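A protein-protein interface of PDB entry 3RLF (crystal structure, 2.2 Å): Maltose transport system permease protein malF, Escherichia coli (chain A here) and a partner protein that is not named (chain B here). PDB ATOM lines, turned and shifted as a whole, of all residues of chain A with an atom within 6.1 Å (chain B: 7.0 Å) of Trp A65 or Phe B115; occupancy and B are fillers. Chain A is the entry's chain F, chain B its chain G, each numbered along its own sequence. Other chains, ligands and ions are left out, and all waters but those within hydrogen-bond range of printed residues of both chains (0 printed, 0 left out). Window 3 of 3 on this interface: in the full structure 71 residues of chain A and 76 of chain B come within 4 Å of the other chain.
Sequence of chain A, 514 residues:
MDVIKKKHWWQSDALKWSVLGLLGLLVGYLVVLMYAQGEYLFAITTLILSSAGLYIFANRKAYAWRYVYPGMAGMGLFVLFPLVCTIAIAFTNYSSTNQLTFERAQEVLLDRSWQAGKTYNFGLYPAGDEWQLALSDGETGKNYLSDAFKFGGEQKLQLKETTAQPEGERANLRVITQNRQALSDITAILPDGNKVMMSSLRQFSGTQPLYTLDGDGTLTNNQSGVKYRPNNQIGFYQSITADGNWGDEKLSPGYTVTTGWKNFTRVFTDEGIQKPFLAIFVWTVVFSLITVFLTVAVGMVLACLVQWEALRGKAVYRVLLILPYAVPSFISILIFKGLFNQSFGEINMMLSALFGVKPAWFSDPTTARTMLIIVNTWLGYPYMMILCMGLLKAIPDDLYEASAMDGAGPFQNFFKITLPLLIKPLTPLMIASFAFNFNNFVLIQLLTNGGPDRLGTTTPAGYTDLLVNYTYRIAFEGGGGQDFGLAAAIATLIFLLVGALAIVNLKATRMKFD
The backbone carbonyl oxygen of Tyr A67 lies within hydrogen-bond range of the backbone NH of Cys B106, at 3.3 Å.
Hydrophobic or aromatic side chains of chain A within 4 Å of the printed part of chain B: Tyr A63, Ala A64, Trp A65, Tyr A67, Val A68 and Met A72.
Along chain A the printed residues that touch a printed residue of chain B span positions 63 to 72.
Hydrophobic or aromatic side chains of chain B within 4 Å of the printed part of chain A: Tyr B108, Ala B109, Phe B110, Met B113, Phe B115 and Leu B121.
Among the printed residues, 12 pairs touch across the chains.
The backbone carbonyl oxygen (O) of Met B113 is in hydrogen-bond range of the side-chain amino group (NZ) of Lys B118, 3.4 Å away.
The backbone carbonyl oxygen (O) of Phe B110 sits at hydrogen-bond distance from the side-chain amino group (NZ) of Lys B118 (3.3 Å).
The side-chain hydroxyl (OH) of Tyr A63 lies within hydrogen-bond range of the side-chain hydroxyl (OH) of Tyr A67 (3.0 Å).
CE1 of Tyr A63 touches CE of Met B113, 3.6 Å away.
Ala B109 touches Ala A64.
Met B113 touches Ala A64.
Ala A64 touches Phe B115 (CB to CD2, 3.9 Å).
Phe B115 touches Trp A65 (CD1 to CZ2, 3.8 Å).
CD2 of Tyr B108 touches CE2 of Tyr A67, at 3.6 Å.
Tyr A67 touches Ala B109.
Met B113 touches Tyr A67 (CE to CE1, 3.6 Å).
Ala B109 touches Val A68 (CB to CG2, 3.6 Å).
CD2 of Leu B121 touches SD of Met A72 (3.8 Å).
Of the printed residues of chain B, Tyr A63 touches Met B113.
Of the printed residues of chain B, Ala A64 touches Ala B109, Met B113 and Phe B115.
Arg A66 touches none of the printed residues of chain B.
Of the printed residues of chain B, Val A68 touches Ala B109 (3.6 Å) and Phe B110 (3.97 Å).
Printed residues of chain B within 4 Å of Met A72: Leu B121 (3.8 Å).
Phe B115 touches two residues of chain A.
Pro B116 touches none of the printed residues of chain A.
Of the printed residues of chain A, Leu B121 touches Met A72 (3.8 Å).
The nearest printed residue of chain A that does not touch Phe B110 is Met A72 (5.5 Å).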
ATOM      1  N   ILE A  56       8.587 -18.743   9.651  1.00  0.00           N
ATOM      2  CA  ILE A  56       8.951 -19.148   8.290  1.00  0.00           C
ATOM      3  C   ILE A  56       8.505 -18.100   7.263  1.00  0.00           C
ATOM      4  O   ILE A  56       9.273 -17.724   6.375  1.00  0.00           O
ATOM      5  CB  ILE A  56       8.413 -20.571   7.953  1.00  0.00           C
ATOM      6  CG1 ILE A  56       9.352 -21.640   8.522  1.00  0.00           C
ATOM      7  CG2 ILE A  56       8.261 -20.775   6.451  1.00  0.00           C
ATOM      8  CD1 ILE A  56       8.744 -23.038   8.598  1.00  0.00           C
ATOM      9  N   LYS A  61      14.976 -15.459   4.728  1.00  0.00           N
ATOM     10  CA  LYS A  61      16.005 -16.501   4.799  1.00  0.00           C
ATOM     11  C   LYS A  61      15.437 -17.912   4.985  1.00  0.00           C
ATOM     12  O   LYS A  61      16.133 -18.902   4.751  1.00  0.00           O
ATOM     13  CB  LYS A  61      17.041 -16.175   5.880  1.00  0.00           C
ATOM     14  CG  LYS A  61      18.047 -15.119   5.448  1.00  0.00           C
ATOM     15  CD  LYS A  61      19.063 -14.805   6.531  1.00  0.00           C
ATOM     16  CE  LYS A  61      20.076 -13.784   6.030  1.00  0.00           C
ATOM     17  NZ  LYS A  61      21.039 -13.361   7.085  1.00  0.00           N
ATOM     18  N   ALA A  62      14.174 -17.995   5.393  1.00  0.00           N
ATOM     19  CA  ALA A  62      13.484 -19.277   5.514  1.00  0.00           C
ATOM     20  C   ALA A  62      12.501 -19.507   4.355  1.00  0.00           C
ATOM     21  O   ALA A  62      11.457 -20.140   4.528  1.00  0.00           O
ATOM     22  CB  ALA A  62      12.773 -19.366   6.859  1.00  0.00           C
ATOM     23  N   TYR A  63      12.860 -19.002   3.175  1.00  0.00           N
ATOM     24  CA  TYR A  63      12.006 -19.064   1.985  1.00  0.00           C
ATOM     25  C   TYR A  63      11.675 -20.493   1.562  1.00  0.00           C
ATOM     26  O   TYR A  63      10.511 -20.811   1.310  1.00  0.00           O
ATOM     27  CB  TYR A  63      12.649 -18.300   0.819  1.00  0.00           C
ATOM     28  CG  TYR A  63      11.802 -18.226  -0.436  1.00  0.00           C
ATOM     29  CD1 TYR A  63      12.055 -19.065  -1.522  1.00  0.00           C
ATOM     30  CD2 TYR A  63      10.753 -17.311  -0.544  1.00  0.00           C
ATOM     31  CE1 TYR A  63      11.284 -18.999  -2.681  1.00  0.00           C
ATOM     32  CE2 TYR A  63       9.974 -17.237  -1.699  1.00  0.00           C
ATOM     33  CZ  TYR A  63      10.246 -18.084  -2.762  1.00  0.00           C
ATOM     34  OH  TYR A  63       9.484 -18.015  -3.908  1.00  0.00           O
ATOM     35  N   ALA A  64      12.695 -21.347   1.495  1.00  0.00           N
ATOM     36  CA  ALA A  64      12.531 -22.738   1.062  1.00  0.00           C
ATOM     37  C   ALA A  64      11.570 -23.521   1.959  1.00  0.00           C
ATOM     38  O   ALA A  64      10.908 -24.456   1.503  1.00  0.00           O
ATOM     39  CB  ALA A  64      13.881 -23.437   0.988  1.00  0.00           C
ATOM     40  N   TRP A  65      11.494 -23.119   3.225  1.00  0.00           N
ATOM     41  CA  TRP A  65      10.636 -23.780   4.205  1.00  0.00           C
ATOM     42  C   TRP A  65       9.155 -23.441   4.033  1.00  0.00           C
ATOM     43  O   TRP A  65       8.298 -24.132   4.574  1.00  0.00           O
ATOM     44  CB  TRP A  65      11.111 -23.468   5.626  1.00  0.00           C
ATOM     45  CG  TRP A  65      12.474 -24.018   5.918  1.00  0.00           C
ATOM     46  CD1 TRP A  65      13.665 -23.357   5.810  1.00  0.00           C
ATOM     47  CD2 TRP A  65      12.790 -25.346   6.350  1.00  0.00           C
ATOM     48  NE1 TRP A  65      14.703 -24.189   6.153  1.00  0.00           N
ATOM     49  CE2 TRP A  65      14.195 -25.417   6.489  1.00  0.00           C
ATOM     50  CE3 TRP A  65      12.022 -26.485   6.635  1.00  0.00           C
ATOM     51  CZ2 TRP A  65      14.851 -26.581   6.902  1.00  0.00           C
ATOM     52  CZ3 TRP A  65      12.675 -27.644   7.046  1.00  0.00           C
ATOM     53  CH2 TRP A  65      14.077 -27.681   7.176  1.00  0.00           C
ATOM     54  N   ARG A  66       8.860 -22.390   3.269  1.00  0.00           N
ATOM     55  CA  ARG A  66       7.478 -22.020   2.937  1.00  0.00           C
ATOM     56  C   ARG A  66       6.804 -23.056   2.039  1.00  0.00           C
ATOM     57  O   ARG A  66       5.587 -23.242   2.099  1.00  0.00           O
ATOM     58  CB  ARG A  66       7.431 -20.644   2.267  1.00  0.00           C
ATOM     59  CG  ARG A  66       8.019 -19.523   3.112  1.00  0.00           C
ATOM     60  CD  ARG A  66       8.121 -18.216   2.351  1.00  0.00           C
ATOM     61  NE  ARG A  66       8.654 -17.162   3.210  1.00  0.00           N
ATOM     62  CZ  ARG A  66       8.698 -15.871   2.897  1.00  0.00           C
ATOM     63  NH1 ARG A  66       8.236 -15.438   1.730  1.00  0.00           N
ATOM     64  NH2 ARG A  66       9.203 -15.005   3.766  1.00  0.00           N
ATOM     65  N   TYR A  67       7.604 -23.722   1.212  1.00  0.00           N
ATOM     66  CA  TYR A  67       7.114 -24.755   0.297  1.00  0.00           C
ATOM     67  C   TYR A  67       6.932 -26.095   0.994  1.00  0.00           C
ATOM     68  O   TYR A  67       6.180 -26.945   0.526  1.00  0.00           O
ATOM     69  CB  TYR A  67       8.083 -24.927  -0.875  1.00  0.00           C
ATOM     70  CG  TYR A  67       8.074 -23.778  -1.847  1.00  0.00           C
ATOM     71  CD1 TYR A  67       8.789 -22.610  -1.581  1.00  0.00           C
ATOM     72  CD2 TYR A  67       7.353 -23.855  -3.035  1.00  0.00           C
ATOM     73  CE1 TYR A  67       8.779 -21.550  -2.470  1.00  0.00           C
ATOM     74  CE2 TYR A  67       7.340 -22.798  -3.931  1.00  0.00           C
ATOM     75  CZ  TYR A  67       8.055 -21.654  -3.643  1.00  0.00           C
ATOM     76  OH  TYR A  67       8.047 -20.605  -4.523  1.00  0.00           O
ATOM     77  N   VAL A  68       7.630 -26.265   2.113  1.00  0.00           N
ATOM     78  CA  VAL A  68       7.719 -27.544   2.814  1.00  0.00           C
ATOM     79  C   VAL A  68       6.794 -27.599   4.037  1.00  0.00           C
ATOM     80  O   VAL A  68       6.214 -28.645   4.339  1.00  0.00           O
ATOM     81  CB  VAL A  68       9.203 -27.837   3.197  1.00  0.00           C
ATOM     82  CG1 VAL A  68       9.319 -28.907   4.261  1.00  0.00           C
ATOM     83  CG2 VAL A  68      10.000 -28.239   1.964  1.00  0.00           C
ATOM     84  N   TYR A  69       6.650 -26.460   4.716  1.00  0.00           N
ATOM     85  CA  TYR A  69       5.882 -26.359   5.966  1.00  0.00           C
ATOM     86  C   TYR A  69       4.443 -26.902   5.923  1.00  0.00           C
ATOM     87  O   TYR A  69       4.081 -27.712   6.774  1.00  0.00           O
ATOM     88  CB  TYR A  69       5.911 -24.918   6.506  1.00  0.00           C
ATOM     89  CG  TYR A  69       5.012 -24.673   7.696  1.00  0.00           C
ATOM     90  CD1 TYR A  69       3.742 -24.121   7.529  1.00  0.00           C
ATOM     91  CD2 TYR A  69       5.429 -24.993   8.988  1.00  0.00           C
ATOM     92  CE1 TYR A  69       2.907 -23.895   8.614  1.00  0.00           C
ATOM     93  CE2 TYR A  69       4.600 -24.771  10.085  1.00  0.00           C
ATOM     94  CZ  TYR A  69       3.340 -24.223   9.887  1.00  0.00           C
ATOM     95  OH  TYR A  69       2.510 -23.998  10.959  1.00  0.00           O
ATOM     96  N   PRO A  70       3.621 -26.467   4.941  1.00  0.00           N
ATOM     97  CA  PRO A  70       2.227 -26.934   4.939  1.00  0.00           C
ATOM     98  C   PRO A  70       2.101 -28.461   4.838  1.00  0.00           C
ATOM     99  O   PRO A  70       1.282 -29.059   5.542  1.00  0.00           O
ATOM    100  CB  PRO A  70       1.631 -26.257   3.697  1.00  0.00           C
ATOM    101  CG  PRO A  70       2.540 -25.124   3.391  1.00  0.00           C
ATOM    102  CD  PRO A  70       3.895 -25.598   3.781  1.00  0.00           C
ATOM    103  N   MET A  72       4.498 -30.713   5.692  1.00  0.00           N
ATOM    104  CA  MET A  72       5.055 -31.314   6.907  1.00  0.00           C
ATOM    105  C   MET A  72       4.120 -31.186   8.107  1.00  0.00           C
ATOM    106  O   MET A  72       4.142 -32.027   9.004  1.00  0.00           O
ATOM    107  CB  MET A  72       6.425 -30.726   7.248  1.00  0.00           C
ATOM    108  CG  MET A  72       7.531 -31.145   6.297  1.00  0.00           C
ATOM    109  SD  MET A  72       9.171 -31.261   7.055  1.00  0.00           S
ATOM    110  CE  MET A  72       9.308 -29.711   7.957  1.00  0.00           C
ATOM    111  N   CYS B 106       5.959 -29.015  -1.977  1.00  0.00           N
ATOM    112  CA  CYS B 106       6.943 -29.741  -1.181  1.00  0.00           C
ATOM    113  C   CYS B 106       8.069 -30.297  -2.057  1.00  0.00           C
ATOM    114  O   CYS B 106       9.247 -30.116  -1.747  1.00  0.00           O
ATOM    115  CB  CYS B 106       6.247 -30.883  -0.439  1.00  0.00           C
ATOM    116  SG  CYS B 106       6.858 -31.200   1.215  1.00  0.00           S
ATOM    117  N   TYR B 108       8.997 -29.368  -5.024  1.00  0.00           N
ATOM    118  CA  TYR B 108       9.743 -28.295  -5.671  1.00  0.00           C
ATOM    119  C   TYR B 108      10.928 -27.842  -4.818  1.00  0.00           C
ATOM    120  O   TYR B 108      12.033 -27.669  -5.332  1.00  0.00           O
ATOM    121  CB  TYR B 108       8.824 -27.112  -5.998  1.00  0.00           C
ATOM    122  CG  TYR B 108       9.518 -25.933  -6.647  1.00  0.00           C
ATOM    123  CD1 TYR B 108      10.168 -26.071  -7.872  1.00  0.00           C
ATOM    124  CD2 TYR B 108       9.514 -24.678  -6.043  1.00  0.00           C
ATOM    125  CE1 TYR B 108      10.803 -24.994  -8.479  1.00  0.00           C
ATOM    126  CE2 TYR B 108      10.145 -23.592  -6.640  1.00  0.00           C
ATOM    127  CZ  TYR B 108      10.787 -23.759  -7.858  1.00  0.00           C
ATOM    128  OH  TYR B 108      11.412 -22.693  -8.455  1.00  0.00           O
ATOM    129  N   ALA B 109      10.693 -27.659  -3.521  1.00  0.00           N
ATOM    130  CA  ALA B 109      11.764 -27.297  -2.593  1.00  0.00           C
ATOM    131  C   ALA B 109      12.810 -28.408  -2.495  1.00  0.00           C
ATOM    132  O   ALA B 109      14.012 -28.137  -2.505  1.00  0.00           O
ATOM    133  CB  ALA B 109      11.201 -26.969  -1.225  1.00  0.00           C
ATOM    134  N   PHE B 110      12.345 -29.654  -2.424  1.00  0.00           N
ATOM    135  CA  PHE B 110      13.238 -30.804  -2.321  1.00  0.00           C
ATOM    136  C   PHE B 110      14.066 -31.060  -3.586  1.00  0.00           C
ATOM    137  O   PHE B 110      15.124 -31.684  -3.517  1.00  0.00           O
ATOM    138  CB  PHE B 110      12.463 -32.062  -1.922  1.00  0.00           C
ATOM    139  CG  PHE B 110      12.170 -32.157  -0.446  1.00  0.00           C
ATOM    140  CD1 PHE B 110      10.873 -32.033   0.027  1.00  0.00           C
ATOM    141  CD2 PHE B 110      13.195 -32.370   0.469  1.00  0.00           C
ATOM    142  CE1 PHE B 110      10.596 -32.120   1.388  1.00  0.00           C
ATOM    143  CE2 PHE B 110      12.929 -32.463   1.832  1.00  0.00           C
ATOM    144  CZ  PHE B 110      11.626 -32.336   2.291  1.00  0.00           C
ATOM    145  N   ALA B 111      13.585 -30.578  -4.730  1.00  0.00           N
ATOM    146  CA  ALA B 111      14.261 -30.803  -6.011  1.00  0.00           C
ATOM    147  C   ALA B 111      15.121 -29.631  -6.485  1.00  0.00           C
ATOM    148  O   ALA B 111      16.067 -29.832  -7.252  1.00  0.00           O
ATOM    149  CB  ALA B 111      13.244 -31.185  -7.093  1.00  0.00           C
ATOM    150  N   MET B 113      15.685 -26.454  -4.241  1.00  0.00           N
ATOM    151  CA  MET B 113      16.186 -25.582  -3.174  1.00  0.00           C
ATOM    152  C   MET B 113      17.047 -26.320  -2.150  1.00  0.00           C
ATOM    153  O   MET B 113      16.866 -27.516  -1.915  1.00  0.00           O
ATOM    154  CB  MET B 113      15.029 -24.872  -2.470  1.00  0.00           C
ATOM    155  CG  MET B 113      14.259 -23.909  -3.354  1.00  0.00           C
ATOM    156  SD  MET B 113      12.709 -23.406  -2.591  1.00  0.00           S
ATOM    157  CE  MET B 113      12.024 -22.364  -3.867  1.00  0.00           C
ATOM    158  N   ARG B 114      17.979 -25.588  -1.545  1.00  0.00           N
ATOM    159  CA  ARG B 114      18.875 -26.150  -0.536  1.00  0.00           C
ATOM    160  C   ARG B 114      18.495 -25.696   0.869  1.00  0.00           C
ATOM    161  O   ARG B 114      18.246 -24.513   1.105  1.00  0.00           O
ATOM    162  CB  ARG B 114      20.336 -25.795  -0.841  1.00  0.00           C
ATOM    163  CG  ARG B 114      20.882 -26.468  -2.094  1.00  0.00           C
ATOM    164  CD  ARG B 114      22.370 -26.208  -2.291  1.00  0.00           C
ATOM    165  NE  ARG B 114      22.843 -26.792  -3.548  1.00  0.00           N
ATOM    166  CZ  ARG B 114      24.107 -26.788  -3.964  1.00  0.00           C
ATOM    167  NH1 ARG B 114      25.063 -26.228  -3.228  1.00  0.00           N
ATOM    168  NH2 ARG B 114      24.420 -27.348  -5.127  1.00  0.00           N
ATOM    169  N   PHE B 115      18.439 -26.658   1.787  1.00  0.00           N
ATOM    170  CA  PHE B 115      18.192 -26.401   3.206  1.00  0.00           C
ATOM    171  C   PHE B 115      18.752 -27.549   4.054  1.00  0.00           C
ATOM    172  O   PHE B 115      18.831 -28.683   3.573  1.00  0.00           O
ATOM    173  CB  PHE B 115      16.699 -26.157   3.496  1.00  0.00           C
ATOM    174  CG  PHE B 115      15.773 -27.193   2.914  1.00  0.00           C
ATOM    175  CD1 PHE B 115      15.441 -28.336   3.636  1.00  0.00           C
ATOM    176  CD2 PHE B 115      15.211 -27.010   1.652  1.00  0.00           C
ATOM    177  CE1 PHE B 115      14.579 -29.291   3.103  1.00  0.00           C
ATOM    178  CE2 PHE B 115      14.349 -27.959   1.110  1.00  0.00           C
ATOM    179  CZ  PHE B 115      14.031 -29.102   1.837  1.00  0.00           C
ATOM    180  N   PRO B 116      19.156 -27.257   5.309  1.00  0.00           N
ATOM    181  CA  PRO B 116      19.808 -28.255   6.166  1.00  0.00           C
ATOM    182  C   PRO B 116      18.956 -29.500   6.416  1.00  0.00           C
ATOM    183  O   PRO B 116      17.769 -29.388   6.739  1.00  0.00           O
ATOM    184  CB  PRO B 116      20.044 -27.493   7.480  1.00  0.00           C
ATOM    185  CG  PRO B 116      19.094 -26.341   7.439  1.00  0.00           C
ATOM    186  CD  PRO B 116      19.033 -25.958   5.998  1.00  0.00           C
ATOM    187  N   GLY B 117      19.572 -30.671   6.254  1.00  0.00           N
ATOM    188  CA  GLY B 117      18.904 -31.954   6.479  1.00  0.00           C
ATOM    189  C   GLY B 117      17.848 -32.287   5.442  1.00  0.00           C
ATOM    190  O   GLY B 117      16.768 -32.775   5.782  1.00  0.00           O
ATOM    191  N   LYS B 118      18.166 -32.025   4.175  1.00  0.00           N
ATOM    192  CA  LYS B 118      17.241 -32.261   3.066  1.00  0.00           C
ATOM    193  C   LYS B 118      17.053 -33.753   2.800  1.00  0.00           C
ATOM    194  O   LYS B 118      15.926 -34.220   2.625  1.00  0.00           O
ATOM    195  CB  LYS B 118      17.727 -31.548   1.799  1.00  0.00           C
ATOM    196  CG  LYS B 118      16.676 -31.450   0.698  1.00  0.00           C
ATOM    197  CD  LYS B 118      17.122 -30.566  -0.458  1.00  0.00           C
ATOM    198  CE  LYS B 118      17.853 -31.356  -1.531  1.00  0.00           C
ATOM    199  NZ  LYS B 118      18.113 -30.528  -2.743  1.00  0.00           N
ATOM    200  N   ALA B 119      18.163 -34.489   2.777  1.00  0.00           N
ATOM    201  CA  ALA B 119      18.147 -35.929   2.528  1.00  0.00           C
ATOM    202  C   ALA B 119      17.591 -36.717   3.714  1.00  0.00           C
ATOM    203  O   ALA B 119      16.993 -37.778   3.526  1.00  0.00           O
ATOM    204  CB  ALA B 119      19.540 -36.421   2.164  1.00  0.00           C
ATOM    205  N   LEU B 121      15.178 -35.614   6.004  1.00  0.00           N
ATOM    206  CA  LEU B 121      13.722 -35.436   6.039  1.00  0.00           C
ATOM    207  C   LEU B 121      13.000 -36.223   4.951  1.00  0.00           C
ATOM    208  O   LEU B 121      11.916 -36.746   5.191  1.00  0.00           O
ATOM    209  CB  LEU B 121      13.347 -33.952   5.958  1.00  0.00           C
ATOM    210  CG  LEU B 121      13.440 -33.139   7.253  1.00  0.00           C
ATOM    211  CD1 LEU B 121      13.715 -31.672   6.951  1.00  0.00           C
ATOM    212  CD2 LEU B 121      12.180 -33.294   8.103  1.00  0.00           C
ATOM    213  N   LEU B 122      13.602 -36.303   3.765  1.00  0.00           N
ATOM    214  CA  LEU B 122      13.056 -37.102   2.665  1.00  0.00           C
ATOM    215  C   LEU B 122      12.962 -38.575   3.041  1.00  0.00           C
ATOM    216  O   LEU B 122      11.921 -39.203   2.839  1.00  0.00           O
ATOM    217  CB  LEU B 122      13.903 -36.948   1.401  1.00  0.00           C
ATOM    218  CG  LEU B 122      13.483 -35.890   0.386  1.00  0.00           C
ATOM    219  CD1 LEU B 122      14.646 -35.569  -0.537  1.00  0.00           C
ATOM    220  CD2 LEU B 122      12.264 -36.342  -0.412  1.00  0.00           C
